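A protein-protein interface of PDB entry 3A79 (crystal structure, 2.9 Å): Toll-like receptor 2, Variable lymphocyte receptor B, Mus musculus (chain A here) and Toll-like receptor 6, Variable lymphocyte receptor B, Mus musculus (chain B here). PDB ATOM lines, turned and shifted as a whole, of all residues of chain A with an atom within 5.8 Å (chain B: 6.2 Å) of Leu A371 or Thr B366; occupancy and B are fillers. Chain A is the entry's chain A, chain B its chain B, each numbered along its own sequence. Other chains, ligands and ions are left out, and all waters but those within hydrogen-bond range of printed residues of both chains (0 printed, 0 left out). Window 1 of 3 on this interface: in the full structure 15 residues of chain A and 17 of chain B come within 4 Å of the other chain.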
ATOM      1  N   PHE A 322      36.643  17.814 -25.915  1.00  0.00           N
ATOM      2  CA  PHE A 322      36.392  17.452 -24.534  1.00  0.00           C
ATOM      3  C   PHE A 322      36.468  15.937 -24.298  1.00  0.00           C
ATOM      4  O   PHE A 322      36.954  15.503 -23.253  1.00  0.00           O
ATOM      5  CB  PHE A 322      35.046  18.010 -24.090  1.00  0.00           C
ATOM      6  CG  PHE A 322      33.878  17.162 -24.490  1.00  0.00           C
ATOM      7  CD1 PHE A 322      33.370  16.202 -23.627  1.00  0.00           C
ATOM      8  CD2 PHE A 322      33.292  17.313 -25.727  1.00  0.00           C
ATOM      9  CE1 PHE A 322      32.303  15.406 -24.002  1.00  0.00           C
ATOM     10  CE2 PHE A 322      32.220  16.519 -26.103  1.00  0.00           C
ATOM     11  CZ  PHE A 322      31.728  15.567 -25.245  1.00  0.00           C
ATOM     12  N   LYS A 347      31.167  20.204 -19.574  1.00  0.00           N
ATOM     13  CA  LYS A 347      31.059  18.930 -20.262  1.00  0.00           C
ATOM     14  C   LYS A 347      31.725  17.815 -19.478  1.00  0.00           C
ATOM     15  O   LYS A 347      32.207  16.855 -20.061  1.00  0.00           O
ATOM     16  CB  LYS A 347      31.662  19.013 -21.674  1.00  0.00           C
ATOM     17  CG  LYS A 347      31.036  20.065 -22.595  1.00  0.00           C
ATOM     18  CD  LYS A 347      30.938  19.535 -24.020  1.00  0.00           C
ATOM     19  CE  LYS A 347      30.598  20.621 -25.023  1.00  0.00           C
ATOM     20  NZ  LYS A 347      30.526  20.030 -26.370  1.00  0.00           N
ATOM     21  N   VAL A 348      31.753  17.937 -18.156  1.00  0.00           N
ATOM     22  CA  VAL A 348      32.311  16.880 -17.319  1.00  0.00           C
ATOM     23  C   VAL A 348      31.484  15.613 -17.458  1.00  0.00           C
ATOM     24  O   VAL A 348      30.273  15.643 -17.268  1.00  0.00           O
ATOM     25  CB  VAL A 348      32.351  17.301 -15.841  1.00  0.00           C
ATOM     26  CG1 VAL A 348      33.100  16.269 -14.992  1.00  0.00           C
ATOM     27  CG2 VAL A 348      32.981  18.674 -15.716  1.00  0.00           C
ATOM     28  N   PHE A 349      32.126  14.502 -17.796  1.00  0.00           N
ATOM     29  CA  PHE A 349      31.387  13.257 -17.970  1.00  0.00           C
ATOM     30  C   PHE A 349      31.904  12.143 -17.091  1.00  0.00           C
ATOM     31  O   PHE A 349      31.334  11.061 -17.079  1.00  0.00           O
ATOM     32  CB  PHE A 349      31.406  12.795 -19.422  1.00  0.00           C
ATOM     33  CG  PHE A 349      32.778  12.483 -19.937  1.00  0.00           C
ATOM     34  CD1 PHE A 349      33.364  11.247 -19.687  1.00  0.00           C
ATOM     35  CD2 PHE A 349      33.480  13.421 -20.678  1.00  0.00           C
ATOM     36  CE1 PHE A 349      34.636  10.946 -20.167  1.00  0.00           C
ATOM     37  CE2 PHE A 349      34.749  13.136 -21.161  1.00  0.00           C
ATOM     38  CZ  PHE A 349      35.330  11.891 -20.906  1.00  0.00           C
ATOM     39  N   GLU A 369      25.168  20.982 -14.514  1.00  0.00           N
ATOM     40  CA  GLU A 369      25.082  21.256 -15.944  1.00  0.00           C
ATOM     41  C   GLU A 369      26.115  20.482 -16.760  1.00  0.00           C
ATOM     42  O   GLU A 369      26.630  20.973 -17.767  1.00  0.00           O
ATOM     43  CB  GLU A 369      25.238  22.756 -16.187  1.00  0.00           C
ATOM     44  CG  GLU A 369      24.436  23.305 -17.354  1.00  0.00           C
ATOM     45  CD  GLU A 369      24.134  24.790 -17.204  1.00  0.00           C
ATOM     46  OE1 GLU A 369      23.813  25.437 -18.226  1.00  0.00           O
ATOM     47  OE2 GLU A 369      24.215  25.306 -16.061  1.00  0.00           O
ATOM     48  N   ASN A 370      26.412  19.263 -16.337  1.00  0.00           N
ATOM     49  CA  ASN A 370      27.358  18.454 -17.078  1.00  0.00           C
ATOM     50  C   ASN A 370      26.738  17.187 -17.686  1.00  0.00           C
ATOM     51  O   ASN A 370      25.554  17.161 -18.011  1.00  0.00           O
ATOM     52  CB  ASN A 370      28.580  18.142 -16.212  1.00  0.00           C
ATOM     53  CG  ASN A 370      29.411  19.376 -15.908  1.00  0.00           C
ATOM     54  OD1 ASN A 370      29.505  19.813 -14.758  1.00  0.00           O
ATOM     55  ND2 ASN A 370      30.017  19.945 -16.940  1.00  0.00           N
ATOM     56  N   LEU A 371      27.551  16.150 -17.857  1.00  0.00           N
ATOM     57  CA  LEU A 371      27.116  14.931 -18.519  1.00  0.00           C
ATOM     58  C   LEU A 371      27.129  13.696 -17.613  1.00  0.00           C
ATOM     59  O   LEU A 371      27.079  12.573 -18.106  1.00  0.00           O
ATOM     60  CB  LEU A 371      27.996  14.668 -19.736  1.00  0.00           C
ATOM     61  CG  LEU A 371      27.716  15.412 -21.039  1.00  0.00           C
ATOM     62  CD1 LEU A 371      26.999  16.717 -20.801  1.00  0.00           C
ATOM     63  CD2 LEU A 371      29.021  15.638 -21.788  1.00  0.00           C
ATOM     64  N   MET A 372      27.196  13.887 -16.300  1.00  0.00           N
ATOM     65  CA  MET A 372      27.175  12.744 -15.389  1.00  0.00           C
ATOM     66  C   MET A 372      25.898  11.932 -15.538  1.00  0.00           C
ATOM     67  O   MET A 372      24.793  12.467 -15.562  1.00  0.00           O
ATOM     68  CB  MET A 372      27.340  13.171 -13.930  1.00  0.00           C
ATOM     69  CG  MET A 372      28.600  13.968 -13.662  1.00  0.00           C
ATOM     70  SD  MET A 372      30.111  13.041 -13.953  1.00  0.00           S
ATOM     71  CE  MET A 372      30.090  11.885 -12.584  1.00  0.00           C
ATOM     72  N   VAL A 373      26.079  10.626 -15.655  1.00  0.00           N
ATOM     73  CA  VAL A 373      24.987   9.672 -15.652  1.00  0.00           C
ATOM     74  C   VAL A 373      25.367   8.551 -14.676  1.00  0.00           C
ATOM     75  O   VAL A 373      26.547   8.289 -14.463  1.00  0.00           O
ATOM     76  CB  VAL A 373      24.714   9.131 -17.072  1.00  0.00           C
ATOM     77  CG1 VAL A 373      24.067  10.208 -17.912  1.00  0.00           C
ATOM     78  CG2 VAL A 373      26.004   8.657 -17.734  1.00  0.00           C
ATOM     79  N   TYR A 376      28.681   6.669 -15.094  1.00  0.00           N
ATOM     80  CA  TYR A 376      29.925   7.301 -14.690  1.00  0.00           C
ATOM     81  C   TYR A 376      29.964   7.587 -13.197  1.00  0.00           C
ATOM     82  O   TYR A 376      30.960   7.322 -12.529  1.00  0.00           O
ATOM     83  CB  TYR A 376      30.120   8.592 -15.467  1.00  0.00           C
ATOM     84  CG  TYR A 376      30.221   8.341 -16.939  1.00  0.00           C
ATOM     85  CD1 TYR A 376      29.198   8.709 -17.789  1.00  0.00           C
ATOM     86  CD2 TYR A 376      31.334   7.702 -17.479  1.00  0.00           C
ATOM     87  CE1 TYR A 376      29.285   8.466 -19.146  1.00  0.00           C
ATOM     88  CE2 TYR A 376      31.427   7.451 -18.834  1.00  0.00           C
ATOM     89  CZ  TYR A 376      30.399   7.836 -19.661  1.00  0.00           C
ATOM     90  OH  TYR A 376      30.463   7.602 -21.009  1.00  0.00           O
ATOM     91  N   ASN A 397      22.271  17.469 -14.625  1.00  0.00           N
ATOM     92  CA  ASN A 397      22.966  16.444 -15.379  1.00  0.00           C
ATOM     93  C   ASN A 397      21.937  15.554 -16.062  1.00  0.00           C
ATOM     94  O   ASN A 397      20.827  16.004 -16.346  1.00  0.00           O
ATOM     95  CB  ASN A 397      23.954  15.674 -14.504  1.00  0.00           C
ATOM     96  CG  ASN A 397      25.167  16.511 -14.147  1.00  0.00           C
ATOM     97  OD1 ASN A 397      25.084  17.450 -13.361  1.00  0.00           O
ATOM     98  ND2 ASN A 397      26.292  16.190 -14.743  1.00  0.00           N
ATOM     99  N   HIS A 398      22.285  14.310 -16.354  1.00  0.00           N
ATOM    100  CA  HIS A 398      21.364  13.492 -17.126  1.00  0.00           C
ATOM    101  C   HIS A 398      20.934  12.243 -16.382  1.00  0.00           C
ATOM    102  O   HIS A 398      20.716  11.185 -16.975  1.00  0.00           O
ATOM    103  CB  HIS A 398      21.947  13.174 -18.503  1.00  0.00           C
ATOM    104  CG  HIS A 398      21.963  14.354 -19.424  1.00  0.00           C
ATOM    105  ND1 HIS A 398      20.816  14.881 -19.975  1.00  0.00           N
ATOM    106  CD2 HIS A 398      22.983  15.125 -19.868  1.00  0.00           C
ATOM    107  CE1 HIS A 398      21.128  15.920 -20.729  1.00  0.00           C
ATOM    108  NE2 HIS A 398      22.438  16.090 -20.681  1.00  0.00           N
ATOM    109  N   ILE B 344      29.525   9.624 -25.254  1.00  0.00           N
ATOM    110  CA  ILE B 344      29.494  11.076 -25.092  1.00  0.00           C
ATOM    111  C   ILE B 344      29.707  11.819 -26.410  1.00  0.00           C
ATOM    112  O   ILE B 344      29.667  13.056 -26.452  1.00  0.00           O
ATOM    113  CB  ILE B 344      30.582  11.534 -24.119  1.00  0.00           C
ATOM    114  CG1 ILE B 344      31.947  11.080 -24.618  1.00  0.00           C
ATOM    115  CG2 ILE B 344      30.341  10.976 -22.740  1.00  0.00           C
ATOM    116  CD1 ILE B 344      33.091  11.526 -23.729  1.00  0.00           C
ATOM    117  N   HIS B 345      29.921  11.063 -27.485  1.00  0.00           N
ATOM    118  CA  HIS B 345      30.397  11.634 -28.741  1.00  0.00           C
ATOM    119  C   HIS B 345      30.418  10.632 -29.892  1.00  0.00           C
ATOM    120  O   HIS B 345      30.307   9.421 -29.687  1.00  0.00           O
ATOM    121  CB  HIS B 345      31.816  12.175 -28.542  1.00  0.00           C
ATOM    122  CG  HIS B 345      32.225  13.182 -29.569  1.00  0.00           C
ATOM    123  ND1 HIS B 345      31.733  14.469 -29.585  1.00  0.00           N
ATOM    124  CD2 HIS B 345      33.077  13.095 -30.617  1.00  0.00           C
ATOM    125  CE1 HIS B 345      32.265  15.129 -30.596  1.00  0.00           C
ATOM    126  NE2 HIS B 345      33.080  14.316 -31.242  1.00  0.00           N
ATOM    127  N   VAL B 364      24.670  10.379 -24.584  1.00  0.00           N
ATOM    128  CA  VAL B 364      25.055  11.596 -23.898  1.00  0.00           C
ATOM    129  C   VAL B 364      25.889  12.470 -24.844  1.00  0.00           C
ATOM    130  O   VAL B 364      26.919  13.019 -24.451  1.00  0.00           O
ATOM    131  CB  VAL B 364      25.810  11.284 -22.586  1.00  0.00           C
ATOM    132  CG1 VAL B 364      25.757  12.489 -21.635  1.00  0.00           C
ATOM    133  CG2 VAL B 364      25.207  10.040 -21.908  1.00  0.00           C
ATOM    134  N   PHE B 365      25.429  12.588 -26.093  1.00  0.00           N
ATOM    135  CA  PHE B 365      26.091  13.414 -27.114  1.00  0.00           C
ATOM    136  C   PHE B 365      25.999  14.916 -26.833  1.00  0.00           C
ATOM    137  O   PHE B 365      25.106  15.377 -26.134  1.00  0.00           O
ATOM    138  CB  PHE B 365      25.497  13.148 -28.499  1.00  0.00           C
ATOM    139  CG  PHE B 365      25.983  11.881 -29.145  1.00  0.00           C
ATOM    140  CD1 PHE B 365      26.539  10.859 -28.382  1.00  0.00           C
ATOM    141  CD2 PHE B 365      25.851  11.697 -30.524  1.00  0.00           C
ATOM    142  CE1 PHE B 365      26.975   9.698 -28.982  1.00  0.00           C
ATOM    143  CE2 PHE B 365      26.276  10.533 -31.128  1.00  0.00           C
ATOM    144  CZ  PHE B 365      26.843   9.535 -30.361  1.00  0.00           C
ATOM    145  N   THR B 366      26.909  15.683 -27.414  1.00  0.00           N
ATOM    146  CA  THR B 366      26.890  17.125 -27.227  1.00  0.00           C
ATOM    147  C   THR B 366      26.799  17.855 -28.558  1.00  0.00           C
ATOM    148  O   THR B 366      26.832  17.236 -29.620  1.00  0.00           O
ATOM    149  CB  THR B 366      28.121  17.606 -26.437  1.00  0.00           C
ATOM    150  OG1 THR B 366      29.323  17.353 -27.188  1.00  0.00           O
ATOM    151  CG2 THR B 366      28.177  16.889 -25.094  1.00  0.00           C
ATOM    152  N   ASP B 367      26.670  19.173 -28.492  1.00  0.00           N
ATOM    153  CA  ASP B 367      26.548  20.003 -29.684  1.00  0.00           C
ATOM    154  C   ASP B 367      27.848  20.064 -30.483  1.00  0.00           C
ATOM    155  O   ASP B 367      27.872  20.595 -31.596  1.00  0.00           O
ATOM    156  CB  ASP B 367      26.080  21.417 -29.310  1.00  0.00           C
ATOM    157  CG  ASP B 367      26.859  22.000 -28.146  1.00  0.00           C
ATOM    158  OD1 ASP B 367      26.221  22.445 -27.165  1.00  0.00           O
ATOM    159  OD2 ASP B 367      28.111  22.000 -28.209  1.00  0.00           O
ATOM    160  N   SER B 368      28.925  19.524 -29.919  1.00  0.00           N
ATOM    161  CA  SER B 368      30.190  19.462 -30.645  1.00  0.00           C
ATOM    162  C   SER B 368      30.233  18.263 -31.600  1.00  0.00           C
ATOM    163  O   SER B 368      31.127  18.155 -32.435  1.00  0.00           O
ATOM    164  CB  SER B 368      31.387  19.449 -29.693  1.00  0.00           C
ATOM    165  OG  SER B 368      31.333  18.337 -28.829  1.00  0.00           O
ATOM    166  N   VAL B 369      29.254  17.374 -31.485  1.00  0.00           N
ATOM    167  CA  VAL B 369      29.173  16.249 -32.394  1.00  0.00           C
ATOM    168  C   VAL B 369      29.184  16.755 -33.833  1.00  0.00           C
ATOM    169  O   VAL B 369      28.442  17.685 -34.178  1.00  0.00           O
ATOM    170  CB  VAL B 369      27.928  15.372 -32.134  1.00  0.00           C
ATOM    171  CG1 VAL B 369      26.700  15.960 -32.807  1.00  0.00           C
ATOM    172  CG2 VAL B 369      28.176  13.943 -32.619  1.00  0.00           C
ATOM    173  N   PHE B 370      30.047  16.145 -34.649  1.00  0.00           N
ATOM    174  CA  PHE B 370      30.189  16.477 -36.063  1.00  0.00           C
ATOM    175  C   PHE B 370      30.439  17.973 -36.360  1.00  0.00           C
ATOM    176  O   PHE B 370      30.036  18.481 -37.413  1.00  0.00           O
ATOM    177  CB  PHE B 370      28.979  15.976 -36.863  1.00  0.00           C
ATOM    178  CG  PHE B 370      28.711  14.513 -36.708  1.00  0.00           C
ATOM    179  CD1 PHE B 370      27.415  14.033 -36.720  1.00  0.00           C
ATOM    180  CD2 PHE B 370      29.748  13.616 -36.551  1.00  0.00           C
ATOM    181  CE1 PHE B 370      27.153  12.679 -36.580  1.00  0.00           C
ATOM    182  CE2 PHE B 370      29.497  12.256 -36.413  1.00  0.00           C
ATOM    183  CZ  PHE B 370      28.198  11.789 -36.424  1.00  0.00           C
ATOM    184  N   ASN B 387      19.564  13.417 -26.158  1.00  0.00           N
ATOM    185  CA  ASN B 387      20.955  13.645 -25.783  1.00  0.00           C
ATOM    186  C   ASN B 387      21.149  14.962 -25.022  1.00  0.00           C
ATOM    187  O   ASN B 387      20.196  15.502 -24.455  1.00  0.00           O
ATOM    188  CB  ASN B 387      21.848  13.572 -27.021  1.00  0.00           C
ATOM    189  CG  ASN B 387      21.921  12.167 -27.599  1.00  0.00           C
ATOM    190  OD1 ASN B 387      21.193  11.824 -28.537  1.00  0.00           O
ATOM    191  ND2 ASN B 387      22.788  11.342 -27.028  1.00  0.00           N
ATOM    192  N   GLY B 388      22.375  15.478 -25.006  1.00  0.00           N
ATOM    193  CA  GLY B 388      22.671  16.691 -24.262  1.00  0.00           C
ATOM    194  C   GLY B 388      23.029  17.900 -25.105  1.00  0.00           C
ATOM    195  O   GLY B 388      23.847  18.713 -24.686  1.00  0.00           O
ATOM    196  N   LEU B 389      22.434  18.037 -26.289  1.00  0.00           N
ATOM    197  CA  LEU B 389      22.762  19.163 -27.166  1.00  0.00           C
ATOM    198  C   LEU B 389      22.333  20.493 -26.562  1.00  0.00           C
ATOM    199  O   LEU B 389      21.143  20.729 -26.371  1.00  0.00           O
ATOM    200  CB  LEU B 389      22.106  19.006 -28.539  1.00  0.00           C
ATOM    201  CG  LEU B 389      22.448  17.788 -29.384  1.00  0.00           C
ATOM    202  CD1 LEU B 389      22.129  18.053 -30.851  1.00  0.00           C
ATOM    203  CD2 LEU B 389      23.898  17.464 -29.205  1.00  0.00           C
ATOM    204  N   LYS B 390      23.290  21.375 -26.283  1.00  0.00           N
ATOM    205  CA  LYS B 390      22.978  22.631 -25.588  1.00  0.00           C
ATOM    206  C   LYS B 390      22.614  23.775 -26.536  1.00  0.00           C
ATOM    207  O   LYS B 390      21.498  24.289 -26.501  1.00  0.00           O
ATOM    208  CB  LYS B 390      24.156  23.068 -24.712  1.00  0.00           C
ATOM    209  CG  LYS B 390      23.814  23.384 -23.260  1.00  0.00           C
ATOM    210  CD  LYS B 390      23.983  22.143 -22.377  1.00  0.00           C
ATOM    211  CE  LYS B 390      24.277  22.531 -20.941  1.00  0.00           C
ATOM    212  NZ  LYS B 390      23.271  23.511 -20.389  1.00  0.00           N
ATOM    213  N   MET B 398      26.580  22.660 -37.393  1.00  0.00           N
ATOM    214  CA  MET B 398      26.896  21.253 -37.592  1.00  0.00           C
ATOM    215  C   MET B 398      26.534  20.761 -38.988  1.00  0.00           C
ATOM    216  O   MET B 398      27.270  19.989 -39.597  1.00  0.00           O
ATOM    217  CB  MET B 398      26.152  20.411 -36.566  1.00  0.00           C
ATOM    218  CG  MET B 398      26.213  18.918 -36.833  1.00  0.00           C
ATOM    219  SD  MET B 398      25.450  18.007 -35.487  1.00  0.00           S
ATOM    220  CE  MET B 398      23.758  17.901 -36.062  1.00  0.00           C
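The side-chain amino group (NZ) of Lys A347 sits at hydrogen-bond distance from the side-chain hydroxyl (OG) of Ser B368 (3.1 Å).
NZ of Lys A347 sits at hydrogen-bond distance from OG1 of Thr B366, 3.0 Å away.
The side-chain carboxylate (OE1) of Glu A369 is in salt-bridge range of the side-chain amino group (NZ) of Lys B390.
The side-chain amino group of Lys A347 lies within salt-bridge range of the side-chain carboxylate of Asp B367, 3.6 Å away.
N of Gly B388 sits at hydrogen-bond distance from O of Phe B365.
The backbone carbonyl oxygen (O) of Val A348 sits at hydrogen-bond distance from the backbone NH (N) of Leu A371 (2.8 Å).
The side-chain amide nitrogen (ND2) of Asn B387 lies close to the backbone NH (N) of Phe B365 (3.1 Å).
The side-chain amide nitrogen (ND2) of Asn A370 sits close to the backbone NH (N) of Lys A347.
The backbone NH (N) of Lys B390 sits at hydrogen-bond distance from the side-chain carboxylate (OD1) of Asp B367 (3.2 Å).
The backbone NH (N) of Leu A371 sits close to the side-chain amide nitrogen (ND2) of Asn A397.
Ile B344 touches Phe A322.
Phe A322 touches Thr B366 (CE2 to OG1, 3.2 Å).
Phe A322 touches Ser B368 (CE2 to OG, 3.4 Å).
Phe A349 touches Ile B344.
CG of Leu A371 touches CG1 of Val B364, 3.6 Å away.
CD2 of Leu A371 touches CG2 of Thr B366, 3.6 Å away.
Tyr A376 touches Ile B344 (OH to CG2, 3.8 Å).
His A398 touches Asn B387.
Gly B388 touches His A398.
Of chain B, only Val B364 (3.6 Å) and Thr B366 (3.6 Å) come within 4 Å of Leu A371.
Thr B366 touches three residues of chain A.
Of the printed residues of chain A, Gly B388 touches His A398 (3.6 Å).
Of the printed residues of chain B, Lys A347 touches Thr B366 (3.0 Å), Asp B367 (3.6 Å) and Ser B368 (3.1 Å).
Of the printed residues of chain A, Asp B367 touches Lys A347.
Printed residues of chain A within 4 Å of Ile B344: Phe A322, Phe A349 and Tyr A376.
Hydrophobic or aromatic side chains of chain B within 4 Å of the printed part of chain A: Ile B344 and Val B364.
Along chain B the printed residues that touch a printed residue of chain A span positions 344 to 390.
Along chain A the printed residues that touch a printed residue of chain B span positions 322 to 398.
Among the printed residues, 13 pairs touch across the chains.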
